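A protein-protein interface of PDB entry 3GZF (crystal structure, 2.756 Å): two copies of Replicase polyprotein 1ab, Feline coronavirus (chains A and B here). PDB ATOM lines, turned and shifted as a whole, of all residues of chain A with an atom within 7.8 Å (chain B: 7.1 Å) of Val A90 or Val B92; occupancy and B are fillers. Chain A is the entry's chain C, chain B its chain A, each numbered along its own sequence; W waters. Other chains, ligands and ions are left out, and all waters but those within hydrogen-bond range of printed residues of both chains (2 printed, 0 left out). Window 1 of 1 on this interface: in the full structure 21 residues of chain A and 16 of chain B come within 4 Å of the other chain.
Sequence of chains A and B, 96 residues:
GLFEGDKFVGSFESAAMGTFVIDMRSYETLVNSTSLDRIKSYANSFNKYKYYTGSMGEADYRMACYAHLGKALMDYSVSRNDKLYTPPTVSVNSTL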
ATOM      1  N   LYS A  48     -15.244 -17.515  -8.603  1.00  0.00           N
ATOM      2  CA  LYS A  48     -15.782 -17.151  -9.896  1.00  0.00           C
ATOM      3  C   LYS A  48     -15.344 -18.141 -10.964  1.00  0.00           C
ATOM      4  O   LYS A  48     -15.971 -18.220 -12.007  1.00  0.00           O
ATOM      5  CB  LYS A  48     -15.270 -15.755 -10.249  1.00  0.00           C
ATOM      6  CG  LYS A  48     -15.934 -15.031 -11.407  1.00  0.00           C
ATOM      7  CD  LYS A  48     -14.981 -13.950 -11.921  1.00  0.00           C
ATOM      8  CE  LYS A  48     -15.688 -12.833 -12.668  1.00  0.00           C
ATOM      9  NZ  LYS A  48     -16.651 -12.057 -11.811  1.00  0.00           N
ATOM     10  N   TYR A  49     -14.267 -18.888 -10.719  1.00  0.00           N
ATOM     11  CA  TYR A  49     -13.690 -19.768 -11.760  1.00  0.00           C
ATOM     12  C   TYR A  49     -13.348 -21.193 -11.319  1.00  0.00           C
ATOM     13  O   TYR A  49     -13.017 -22.039 -12.161  1.00  0.00           O
ATOM     14  CB  TYR A  49     -12.420 -19.163 -12.374  1.00  0.00           C
ATOM     15  CG  TYR A  49     -12.646 -17.962 -13.259  1.00  0.00           C
ATOM     16  CD1 TYR A  49     -12.171 -16.713 -12.889  1.00  0.00           C
ATOM     17  CD2 TYR A  49     -13.344 -18.075 -14.464  1.00  0.00           C
ATOM     18  CE1 TYR A  49     -12.379 -15.599 -13.696  1.00  0.00           C
ATOM     19  CE2 TYR A  49     -13.558 -16.965 -15.281  1.00  0.00           C
ATOM     20  CZ  TYR A  49     -13.068 -15.733 -14.894  1.00  0.00           C
ATOM     21  OH  TYR A  49     -13.275 -14.638 -15.699  1.00  0.00           O
ATOM     22  N   LYS A  50     -13.329 -21.417 -10.006  1.00  0.00           N
ATOM     23  CA  LYS A  50     -13.121 -22.741  -9.417  1.00  0.00           C
ATOM     24  C   LYS A  50     -13.963 -23.802 -10.129  1.00  0.00           C
ATOM     25  O   LYS A  50     -13.503 -24.914 -10.357  1.00  0.00           O
ATOM     26  CB  LYS A  50     -13.485 -22.689  -7.926  1.00  0.00           C
ATOM     27  CG  LYS A  50     -13.083 -23.914  -7.092  1.00  0.00           C
ATOM     28  CD  LYS A  50     -13.282 -23.671  -5.590  1.00  0.00           C
ATOM     29  CE  LYS A  50     -12.625 -24.779  -4.755  1.00  0.00           C
ATOM     30  NZ  LYS A  50     -12.142 -24.316  -3.408  1.00  0.00           N
ATOM     31  N   TYR A  51     -15.207 -23.470 -10.450  1.00  0.00           N
ATOM     32  CA  TYR A  51     -16.043 -24.395 -11.208  1.00  0.00           C
ATOM     33  C   TYR A  51     -16.700 -23.706 -12.399  1.00  0.00           C
ATOM     34  O   TYR A  51     -17.736 -24.155 -12.905  1.00  0.00           O
ATOM     35  CB  TYR A  51     -17.084 -25.044 -10.291  1.00  0.00           C
ATOM     36  CG  TYR A  51     -16.455 -25.576  -9.031  1.00  0.00           C
ATOM     37  CD1 TYR A  51     -15.511 -26.608  -9.080  1.00  0.00           C
ATOM     38  CD2 TYR A  51     -16.784 -25.042  -7.793  1.00  0.00           C
ATOM     39  CE1 TYR A  51     -14.913 -27.101  -7.916  1.00  0.00           C
ATOM     40  CE2 TYR A  51     -16.204 -25.527  -6.621  1.00  0.00           C
ATOM     41  CZ  TYR A  51     -15.267 -26.557  -6.684  1.00  0.00           C
ATOM     42  OH  TYR A  51     -14.677 -27.022  -5.518  1.00  0.00           O
ATOM     43  N   TYR A  52     -16.077 -22.616 -12.843  1.00  0.00           N
ATOM     44  CA  TYR A  52     -16.659 -21.818 -13.894  1.00  0.00           C
ATOM     45  C   TYR A  52     -17.355 -22.781 -14.810  1.00  0.00           C
ATOM     46  O   TYR A  52     -16.740 -23.713 -15.323  1.00  0.00           O
ATOM     47  CB  TYR A  52     -15.601 -21.039 -14.661  1.00  0.00           C
ATOM     48  CG  TYR A  52     -16.170 -20.162 -15.751  1.00  0.00           C
ATOM     49  CD1 TYR A  52     -16.109 -18.777 -15.667  1.00  0.00           C
ATOM     50  CD2 TYR A  52     -16.779 -20.718 -16.860  1.00  0.00           C
ATOM     51  CE1 TYR A  52     -16.644 -17.968 -16.675  1.00  0.00           C
ATOM     52  CE2 TYR A  52     -17.309 -19.924 -17.866  1.00  0.00           C
ATOM     53  CZ  TYR A  52     -17.239 -18.555 -17.772  1.00  0.00           C
ATOM     54  OH  TYR A  52     -17.775 -17.792 -18.788  1.00  0.00           O
ATOM     55  N   THR A  53     -18.653 -22.571 -14.980  1.00  0.00           N
ATOM     56  CA  THR A  53     -19.422 -23.351 -15.914  1.00  0.00           C
ATOM     57  C   THR A  53     -20.256 -22.418 -16.799  1.00  0.00           C
ATOM     58  O   THR A  53     -20.864 -21.458 -16.317  1.00  0.00           O
ATOM     59  CB  THR A  53     -20.297 -24.325 -15.169  1.00  0.00           C
ATOM     60  OG1 THR A  53     -21.031 -25.107 -16.113  1.00  0.00           O
ATOM     61  CG2 THR A  53     -21.255 -23.571 -14.246  1.00  0.00           C
ATOM     62  N   GLY A  54     -20.265 -22.692 -18.098  1.00  0.00           N
ATOM     63  CA  GLY A  54     -20.947 -21.826 -19.047  1.00  0.00           C
ATOM     64  C   GLY A  54     -20.026 -21.423 -20.180  1.00  0.00           C
ATOM     65  O   GLY A  54     -18.966 -22.013 -20.364  1.00  0.00           O
ATOM     66  N   MET A  56     -17.397 -19.067 -22.156  1.00  0.00           N
ATOM     67  CA  MET A  56     -16.438 -17.983 -21.976  1.00  0.00           C
ATOM     68  C   MET A  56     -16.440 -17.116 -23.143  1.00  0.00           C
ATOM     69  O   MET A  56     -16.325 -17.545 -24.292  1.00  0.00           O
ATOM     70  CB  MET A  56     -15.013 -18.464 -21.783  1.00  0.00           C
ATOM     71  CG  MET A  56     -14.926 -19.489 -20.657  1.00  0.00           C
ATOM     72  SD  MET A  56     -13.341 -20.298 -20.445  1.00  0.00           S
ATOM     73  CE  MET A  56     -13.344 -21.280 -21.912  1.00  0.00           C
ATOM     74  N   ASP A  60     -12.155 -14.933 -20.919  1.00  0.00           N
ATOM     75  CA  ASP A  60     -12.404 -15.715 -19.728  1.00  0.00           C
ATOM     76  C   ASP A  60     -11.446 -16.883 -19.576  1.00  0.00           C
ATOM     77  O   ASP A  60     -11.036 -17.249 -18.478  1.00  0.00           O
ATOM     78  CB  ASP A  60     -13.848 -16.202 -19.753  1.00  0.00           C
ATOM     79  CG  ASP A  60     -14.824 -15.068 -19.569  1.00  0.00           C
ATOM     80  OD1 ASP A  60     -14.550 -14.221 -18.687  1.00  0.00           O
ATOM     81  OD2 ASP A  60     -15.832 -15.011 -20.294  1.00  0.00           O
ATOM     82  N   TYR A  61     -11.081 -17.487 -20.685  1.00  0.00           N
ATOM     83  CA  TYR A  61     -10.165 -18.595 -20.610  1.00  0.00           C
ATOM     84  C   TYR A  61      -8.956 -18.179 -19.785  1.00  0.00           C
ATOM     85  O   TYR A  61      -8.651 -18.751 -18.745  1.00  0.00           O
ATOM     86  CB  TYR A  61      -9.708 -18.970 -22.006  1.00  0.00           C
ATOM     87  CG  TYR A  61      -8.962 -20.245 -21.978  1.00  0.00           C
ATOM     88  CD1 TYR A  61      -9.492 -21.396 -22.512  1.00  0.00           C
ATOM     89  CD2 TYR A  61      -7.746 -20.317 -21.337  1.00  0.00           C
ATOM     90  CE1 TYR A  61      -8.800 -22.573 -22.440  1.00  0.00           C
ATOM     91  CE2 TYR A  61      -7.052 -21.487 -21.265  1.00  0.00           C
ATOM     92  CZ  TYR A  61      -7.575 -22.599 -21.818  1.00  0.00           C
ATOM     93  OH  TYR A  61      -6.854 -23.744 -21.729  1.00  0.00           O
ATOM     94  N   ARG A  62      -8.268 -17.166 -20.294  1.00  0.00           N
ATOM     95  CA  ARG A  62      -7.173 -16.486 -19.627  1.00  0.00           C
ATOM     96  C   ARG A  62      -7.402 -16.259 -18.137  1.00  0.00           C
ATOM     97  O   ARG A  62      -6.607 -16.678 -17.311  1.00  0.00           O
ATOM     98  CB  ARG A  62      -7.031 -15.130 -20.288  1.00  0.00           C
ATOM     99  CG  ARG A  62      -5.644 -14.634 -20.464  1.00  0.00           C
ATOM    100  CD  ARG A  62      -5.708 -13.308 -21.229  1.00  0.00           C
ATOM    101  NE  ARG A  62      -6.552 -13.455 -22.401  1.00  0.00           N
ATOM    102  CZ  ARG A  62      -6.897 -12.454 -23.199  1.00  0.00           C
ATOM    103  NH1 ARG A  62      -6.466 -11.229 -22.939  1.00  0.00           N
ATOM    104  NH2 ARG A  62      -7.676 -12.669 -24.252  1.00  0.00           N
ATOM    105  N   ALA A  64      -9.559 -17.587 -16.226  1.00  0.00           N
ATOM    106  CA  ALA A  64      -9.656 -18.787 -15.445  1.00  0.00           C
ATOM    107  C   ALA A  64      -8.249 -19.155 -14.963  1.00  0.00           C
ATOM    108  O   ALA A  64      -7.990 -19.254 -13.762  1.00  0.00           O
ATOM    109  CB  ALA A  64     -10.295 -19.906 -16.241  1.00  0.00           C
ATOM    110  N   CYS A  65      -7.340 -19.333 -15.912  1.00  0.00           N
ATOM    111  CA  CYS A  65      -5.964 -19.681 -15.613  1.00  0.00           C
ATOM    112  C   CYS A  65      -5.327 -18.725 -14.626  1.00  0.00           C
ATOM    113  O   CYS A  65      -4.830 -19.132 -13.574  1.00  0.00           O
ATOM    114  CB  CYS A  65      -5.156 -19.696 -16.896  1.00  0.00           C
ATOM    115  SG  CYS A  65      -5.650 -21.040 -18.015  1.00  0.00           S
ATOM    116  N   HIS A  68      -6.513 -19.460 -11.267  1.00  0.00           N
ATOM    117  CA  HIS A  68      -6.012 -20.627 -10.566  1.00  0.00           C
ATOM    118  C   HIS A  68      -4.548 -20.432 -10.148  1.00  0.00           C
ATOM    119  O   HIS A  68      -4.180 -20.730  -9.017  1.00  0.00           O
ATOM    120  CB  HIS A  68      -6.199 -21.879 -11.409  1.00  0.00           C
ATOM    121  CG  HIS A  68      -7.626 -22.274 -11.568  1.00  0.00           C
ATOM    122  ND1 HIS A  68      -8.098 -23.514 -11.204  1.00  0.00           N
ATOM    123  CD2 HIS A  68      -8.695 -21.582 -12.030  1.00  0.00           C
ATOM    124  CE1 HIS A  68      -9.398 -23.574 -11.440  1.00  0.00           C
ATOM    125  NE2 HIS A  68      -9.785 -22.410 -11.934  1.00  0.00           N
ATOM    126  N   PRO A  87      -2.184 -25.923 -15.458  1.00  0.00           N
ATOM    127  CA  PRO A  87      -3.372 -25.111 -15.684  1.00  0.00           C
ATOM    128  C   PRO A  87      -4.598 -25.967 -15.446  1.00  0.00           C
ATOM    129  O   PRO A  87      -4.482 -27.188 -15.491  1.00  0.00           O
ATOM    130  CB  PRO A  87      -3.263 -24.734 -17.155  1.00  0.00           C
ATOM    131  CG  PRO A  87      -1.829 -24.996 -17.526  1.00  0.00           C
ATOM    132  CD  PRO A  87      -1.417 -26.158 -16.690  1.00  0.00           C
ATOM    133  N   PRO A  88      -5.755 -25.337 -15.171  1.00  0.00           N
ATOM    134  CA  PRO A  88      -7.009 -26.050 -14.911  1.00  0.00           C
ATOM    135  C   PRO A  88      -7.499 -26.796 -16.155  1.00  0.00           C
ATOM    136  O   PRO A  88      -7.084 -26.495 -17.252  1.00  0.00           O
ATOM    137  CB  PRO A  88      -7.981 -24.923 -14.573  1.00  0.00           C
ATOM    138  CG  PRO A  88      -7.387 -23.697 -15.213  1.00  0.00           C
ATOM    139  CD  PRO A  88      -5.927 -23.875 -15.091  1.00  0.00           C
ATOM    140  N   THR A  89      -8.393 -27.749 -16.022  1.00  0.00           N
ATOM    141  CA  THR A  89      -8.916 -28.387 -17.212  1.00  0.00           C
ATOM    142  C   THR A  89     -10.007 -27.526 -17.826  1.00  0.00           C
ATOM    143  O   THR A  89     -10.934 -27.131 -17.135  1.00  0.00           O
ATOM    144  CB  THR A  89      -9.505 -29.727 -16.838  1.00  0.00           C
ATOM    145  OG1 THR A  89      -8.447 -30.674 -16.709  1.00  0.00           O
ATOM    146  CG2 THR A  89     -10.501 -30.217 -17.892  1.00  0.00           C
ATOM    147  N   VAL A  90      -9.922 -27.230 -19.116  1.00  0.00           N
ATOM    148  CA  VAL A  90     -11.021 -26.506 -19.747  1.00  0.00           C
ATOM    149  C   VAL A  90     -11.669 -27.389 -20.790  1.00  0.00           C
ATOM    150  O   VAL A  90     -11.185 -27.506 -21.889  1.00  0.00           O
ATOM    151  CB  VAL A  90     -10.550 -25.188 -20.386  1.00  0.00           C
ATOM    152  CG1 VAL A  90     -11.672 -24.569 -21.188  1.00  0.00           C
ATOM    153  CG2 VAL A  90     -10.052 -24.225 -19.316  1.00  0.00           C
ATOM    154  N   SER A  91     -12.774 -28.013 -20.444  1.00  0.00           N
ATOM    155  CA  SER A  91     -13.327 -29.062 -21.288  1.00  0.00           C
ATOM    156  C   SER A  91     -14.741 -28.751 -21.752  1.00  0.00           C
ATOM    157  O   SER A  91     -15.431 -27.939 -21.151  1.00  0.00           O
ATOM    158  CB  SER A  91     -13.348 -30.365 -20.505  1.00  0.00           C
ATOM    159  OG  SER A  91     -13.946 -30.139 -19.241  1.00  0.00           O
ATOM    160  N   VAL A  92     -15.181 -29.413 -22.815  1.00  0.00           N
ATOM    161  CA  VAL A  92     -16.517 -29.170 -23.336  1.00  0.00           C
ATOM    162  C   VAL A  92     -17.484 -30.289 -22.990  1.00  0.00           C
ATOM    163  O   VAL A  92     -18.695 -30.098 -23.064  1.00  0.00           O
ATOM    164  CB  VAL A  92     -16.508 -28.937 -24.861  1.00  0.00           C
ATOM    165  CG1 VAL A  92     -17.935 -28.680 -25.381  1.00  0.00           C
ATOM    166  CG2 VAL A  92     -15.591 -27.770 -25.194  1.00  0.00           C
ATOM    167  N   TYR B  52     -14.750 -32.859 -28.603  1.00  0.00           N
ATOM    168  CA  TYR B  52     -13.323 -32.628 -28.452  1.00  0.00           C
ATOM    169  C   TYR B  52     -12.752 -33.447 -27.302  1.00  0.00           C
ATOM    170  O   TYR B  52     -13.455 -33.762 -26.343  1.00  0.00           O
ATOM    171  CB  TYR B  52     -12.982 -31.136 -28.282  1.00  0.00           C
ATOM    172  CG  TYR B  52     -11.483 -30.852 -28.333  1.00  0.00           C
ATOM    173  CD1 TYR B  52     -10.854 -30.529 -29.536  1.00  0.00           C
ATOM    174  CD2 TYR B  52     -10.693 -30.946 -27.179  1.00  0.00           C
ATOM    175  CE1 TYR B  52      -9.480 -30.296 -29.601  1.00  0.00           C
ATOM    176  CE2 TYR B  52      -9.316 -30.699 -27.229  1.00  0.00           C
ATOM    177  CZ  TYR B  52      -8.720 -30.375 -28.446  1.00  0.00           C
ATOM    178  OH  TYR B  52      -7.368 -30.133 -28.510  1.00  0.00           O
ATOM    179  N   THR B  53     -11.473 -33.791 -27.438  1.00  0.00           N
ATOM    180  CA  THR B  53     -10.687 -34.486 -26.426  1.00  0.00           C
ATOM    181  C   THR B  53     -10.458 -33.665 -25.138  1.00  0.00           C
ATOM    182  O   THR B  53      -9.323 -33.279 -24.828  1.00  0.00           O
ATOM    183  CB  THR B  53      -9.317 -34.829 -27.021  1.00  0.00           C
ATOM    184  OG1 THR B  53      -8.487 -33.658 -26.986  1.00  0.00           O
ATOM    185  CG2 THR B  53      -9.487 -35.291 -28.473  1.00  0.00           C
ATOM    186  N   GLY B  54     -11.530 -33.427 -24.379  1.00  0.00           N
ATOM    187  CA  GLY B  54     -11.457 -32.612 -23.165  1.00  0.00           C
ATOM    188  C   GLY B  54     -10.936 -31.216 -23.462  1.00  0.00           C
ATOM    189  O   GLY B  54     -11.444 -30.525 -24.370  1.00  0.00           O
ATOM    190  N   SER B  55      -9.919 -30.820 -22.689  1.00  0.00           N
ATOM    191  CA  SER B  55      -9.183 -29.584 -22.909  1.00  0.00           C
ATOM    192  C   SER B  55      -8.319 -29.852 -24.079  1.00  0.00           C
ATOM    193  O   SER B  55      -7.907 -30.973 -24.337  1.00  0.00           O
ATOM    194  CB  SER B  55      -8.282 -29.343 -21.741  1.00  0.00           C
ATOM    195  OG  SER B  55      -7.332 -30.379 -21.808  1.00  0.00           O
ATOM    196  N   MET B  56      -7.770 -28.743 -24.466  1.00  0.00           N
ATOM    197  CA  MET B  56      -8.507 -27.873 -25.268  1.00  0.00           C
ATOM    198  C   MET B  56      -7.910 -26.611 -24.651  1.00  0.00           C
ATOM    199  O   MET B  56      -8.296 -26.168 -23.554  1.00  0.00           O
ATOM    200  CB  MET B  56      -9.970 -27.990 -24.844  1.00  0.00           C
ATOM    201  CG  MET B  56     -10.765 -26.722 -25.185  1.00  0.00           C
ATOM    202  SD  MET B  56     -11.851 -26.771 -26.631  1.00  0.00           S
ATOM    203  CE  MET B  56     -10.699 -27.183 -27.939  1.00  0.00           C
ATOM    204  N   GLY B  57      -6.937 -26.048 -25.372  1.00  0.00           N
ATOM    205  CA  GLY B  57      -6.153 -24.904 -24.925  1.00  0.00           C
ATOM    206  C   GLY B  57      -6.884 -23.612 -25.171  1.00  0.00           C
ATOM    207  O   GLY B  57      -8.098 -23.599 -25.214  1.00  0.00           O
ATOM    208  N   TYR B  61     -10.034 -23.342 -27.936  1.00  0.00           N
ATOM    209  CA  TYR B  61     -11.357 -22.805 -27.634  1.00  0.00           C
ATOM    210  C   TYR B  61     -11.706 -21.724 -28.644  1.00  0.00           C
ATOM    211  O   TYR B  61     -12.781 -21.732 -29.229  1.00  0.00           O
ATOM    212  CB  TYR B  61     -11.405 -22.235 -26.215  1.00  0.00           C
ATOM    213  CG  TYR B  61     -12.774 -21.754 -25.840  1.00  0.00           C
ATOM    214  CD1 TYR B  61     -13.061 -20.396 -25.724  1.00  0.00           C
ATOM    215  CD2 TYR B  61     -13.802 -22.662 -25.651  1.00  0.00           C
ATOM    216  CE1 TYR B  61     -14.341 -19.968 -25.401  1.00  0.00           C
ATOM    217  CE2 TYR B  61     -15.078 -22.253 -25.332  1.00  0.00           C
ATOM    218  CZ  TYR B  61     -15.359 -20.924 -25.197  1.00  0.00           C
ATOM    219  OH  TYR B  61     -16.652 -20.562 -24.871  1.00  0.00           O
ATOM    220  N   VAL B  90     -18.590 -24.799 -21.485  1.00  0.00           N
ATOM    221  CA  VAL B  90     -17.314 -25.300 -21.012  1.00  0.00           C
ATOM    222  C   VAL B  90     -17.395 -25.752 -19.566  1.00  0.00           C
ATOM    223  O   VAL B  90     -18.303 -25.364 -18.834  1.00  0.00           O
ATOM    224  CB  VAL B  90     -16.251 -24.191 -21.090  1.00  0.00           C
ATOM    225  CG1 VAL B  90     -14.935 -24.690 -20.638  1.00  0.00           C
ATOM    226  CG2 VAL B  90     -16.120 -23.754 -22.493  1.00  0.00           C
ATOM    227  N   SER B  91     -16.443 -26.567 -19.148  1.00  0.00           N
ATOM    228  CA  SER B  91     -16.282 -26.815 -17.741  1.00  0.00           C
ATOM    229  C   SER B  91     -14.851 -26.528 -17.380  1.00  0.00           C
ATOM    230  O   SER B  91     -13.936 -26.954 -18.076  1.00  0.00           O
ATOM    231  CB  SER B  91     -16.623 -28.260 -17.383  1.00  0.00           C
ATOM    232  OG  SER B  91     -17.971 -28.509 -17.663  1.00  0.00           O
ATOM    233  N   VAL B  92     -14.653 -25.807 -16.291  1.00  0.00           N
ATOM    234  CA  VAL B  92     -13.315 -25.592 -15.837  1.00  0.00           C
ATOM    235  C   VAL B  92     -13.049 -26.342 -14.559  1.00  0.00           C
ATOM    236  O   VAL B  92     -13.757 -26.172 -13.581  1.00  0.00           O
ATOM    237  CB  VAL B  92     -12.977 -24.088 -15.656  1.00  0.00           C
ATOM    238  CG1 VAL B  92     -11.594 -23.945 -15.085  1.00  0.00           C
ATOM    239  CG2 VAL B  92     -13.109 -23.389 -16.964  1.00  0.00           C
ATOM    240  N   ASN B  93     -12.006 -27.158 -14.566  1.00  0.00           N
ATOM    241  CA  ASN B  93     -11.631 -27.842 -13.363  1.00  0.00           C
ATOM    242  C   ASN B  93     -10.184 -27.764 -13.009  1.00  0.00           C
ATOM    243  O   ASN B  93      -9.324 -27.810 -13.873  1.00  0.00           O
ATOM    244  CB  ASN B  93     -12.064 -29.279 -13.443  1.00  0.00           C
ATOM    245  CG  ASN B  93     -13.447 -29.445 -12.994  1.00  0.00           C
ATOM    246  OD1 ASN B  93     -13.680 -29.988 -11.914  1.00  0.00           O
ATOM    247  ND2 ASN B  93     -14.404 -28.931 -13.778  1.00  0.00           N
ATOM    248  N   SER B  94      -9.938 -27.682 -11.707  1.00  0.00           N
ATOM    249  CA  SER B  94      -8.590 -27.625 -11.134  1.00  0.00           C
ATOM    250  C   SER B  94      -7.735 -28.883 -11.370  1.00  0.00           C
ATOM    251  O   SER B  94      -8.156 -29.843 -12.018  1.00  0.00           O
ATOM    252  CB  SER B  94      -8.679 -27.344  -9.630  1.00  0.00           C
ATOM    253  OG  SER B  94      -7.387 -27.262  -9.061  1.00  0.00           O
HETATM  254  O   HOH W   1     -16.604 -26.850 -13.326  1.00  0.00           O
HETATM  255  O   HOH W   2      -5.811 -26.061 -11.348  1.00  0.00           O
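The backbone NH (N) of Val B92 is in hydrogen-bond range of the backbone carbonyl oxygen (O) of Tyr A52 (3.1 Å).
O of Ser A91 sits at hydrogen-bond distance from N of Ser B91 (2.6 Å).
The backbone carbonyl oxygen of Met B56 sits at hydrogen-bond distance from the side-chain hydroxyl of Tyr A61, at 3.4 Å.
OH of Tyr B61 sits at hydrogen-bond distance from O of Met A56 (3.1 Å).
O of Gly A54 sits at hydrogen-bond distance from N of Val B90 (3.0 Å).
O of Lys A50 lies close to O of Val B92 (3.5 Å).
The backbone carbonyl oxygen of Thr A89 lies close to the backbone carbonyl oxygen of Ser B91, 3.2 Å away.
The backbone NH of Asn B93 lies within hydrogen-bond range of the backbone carbonyl oxygen of Thr A89.
The side-chain sulfur of Met A56 sits close to the backbone NH of Tyr A61, 3.6 Å away.
The side-chain carboxylate of Asp A60 is in hydrogen-bond range of the side-chain hydroxyl of Tyr A49, at 3.3 Å.
The backbone carbonyl oxygen of Tyr A49 lies within hydrogen-bond range of a ring nitrogen (NE2) of His A68, 3.3 Å away.
Among the printed residues, merely in contact across the chains: Tyr A61 with Gly B57, Val A90 with Ser B55, Pro A88 with Asn B93, Thr A89 with Val B92, Val A90 with Met B56, Ser A91 with Val B90, Val A90 with Val B90, Val A90 with Ser B91, Thr A53 with Val B90, Tyr A51 with Val B92, Met A56 with Val B90, Tyr A49 with Val B92, Pro A88 with Val B92, Ser A91 with Gly B54, Val A90 with Gly B54, His A68 with Val B92, Val A90 with Val B92 and Tyr A52 with Ser B91.
Val A90 touches just these residues of chain B: Gly B54, Ser B55, Met B56, Val B90, Ser B91 and Val B92.
Printed residues of chain A within 4 Å of Ser B55: Val A90 (3.1 Å).
Of the printed residues of chain B, Lys A50 touches Val B92.
Of the printed residues of chain A, Val B90 touches Thr A53, Gly A54, Met A56, Val A90 and Ser A91.
Printed residues of chain A within 4 Å of Gly B57: Tyr A61 (3.0 Å).
Asp A60 touches none of the printed residues of chain B.
The nearest residue of chain A that does not touch Val B92 is Ala A64 (4.4 Å).
The nearest printed residue of chain A that does not touch Val B90 is Tyr A52 (4.2 Å).
Along chain A the printed residues that touch a printed residue of chain B span positions 49 to 91.
Of the 12 printed residues of chain B, 9 touch a printed residue of chain A.
Printed residues of chain B that touch a printed residue of chain A: Gly B54, Ser B55, Met B56, Gly B57, Tyr B61, Val B90, Ser B91, Val B92 and Asn B93.
Among the printed residues, 26 pairs touch across the chains.
Met A56 touches Tyr B61, and with the chains exchanged Tyr A61 touches Met B56.
Met A56 touches Val B90, and with the chains exchanged Val A90 touches Met B56.
Val A90 touches its own counterpart, Val B90.
Val A90 touches Val B92, but with the chains exchanged Val A92 does not touch Val B90 (4.6 Å).
Of the 26 pairs that touch across the chains among the printed residues, 10 have their exchanged pair printed and touching as well.
Water W1 lies within hydrogen-bond range of O of Val B92 (2.9 Å), O of Tyr A51 (3.0 Å) and ND2 of Asn B93 (3.1 Å).
Water W2 lies within hydrogen-bond range of the side-chain hydroxyl of Ser B94 (3.0 Å) and a ring nitrogen (ND1) of His A68 (3.4 Å).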
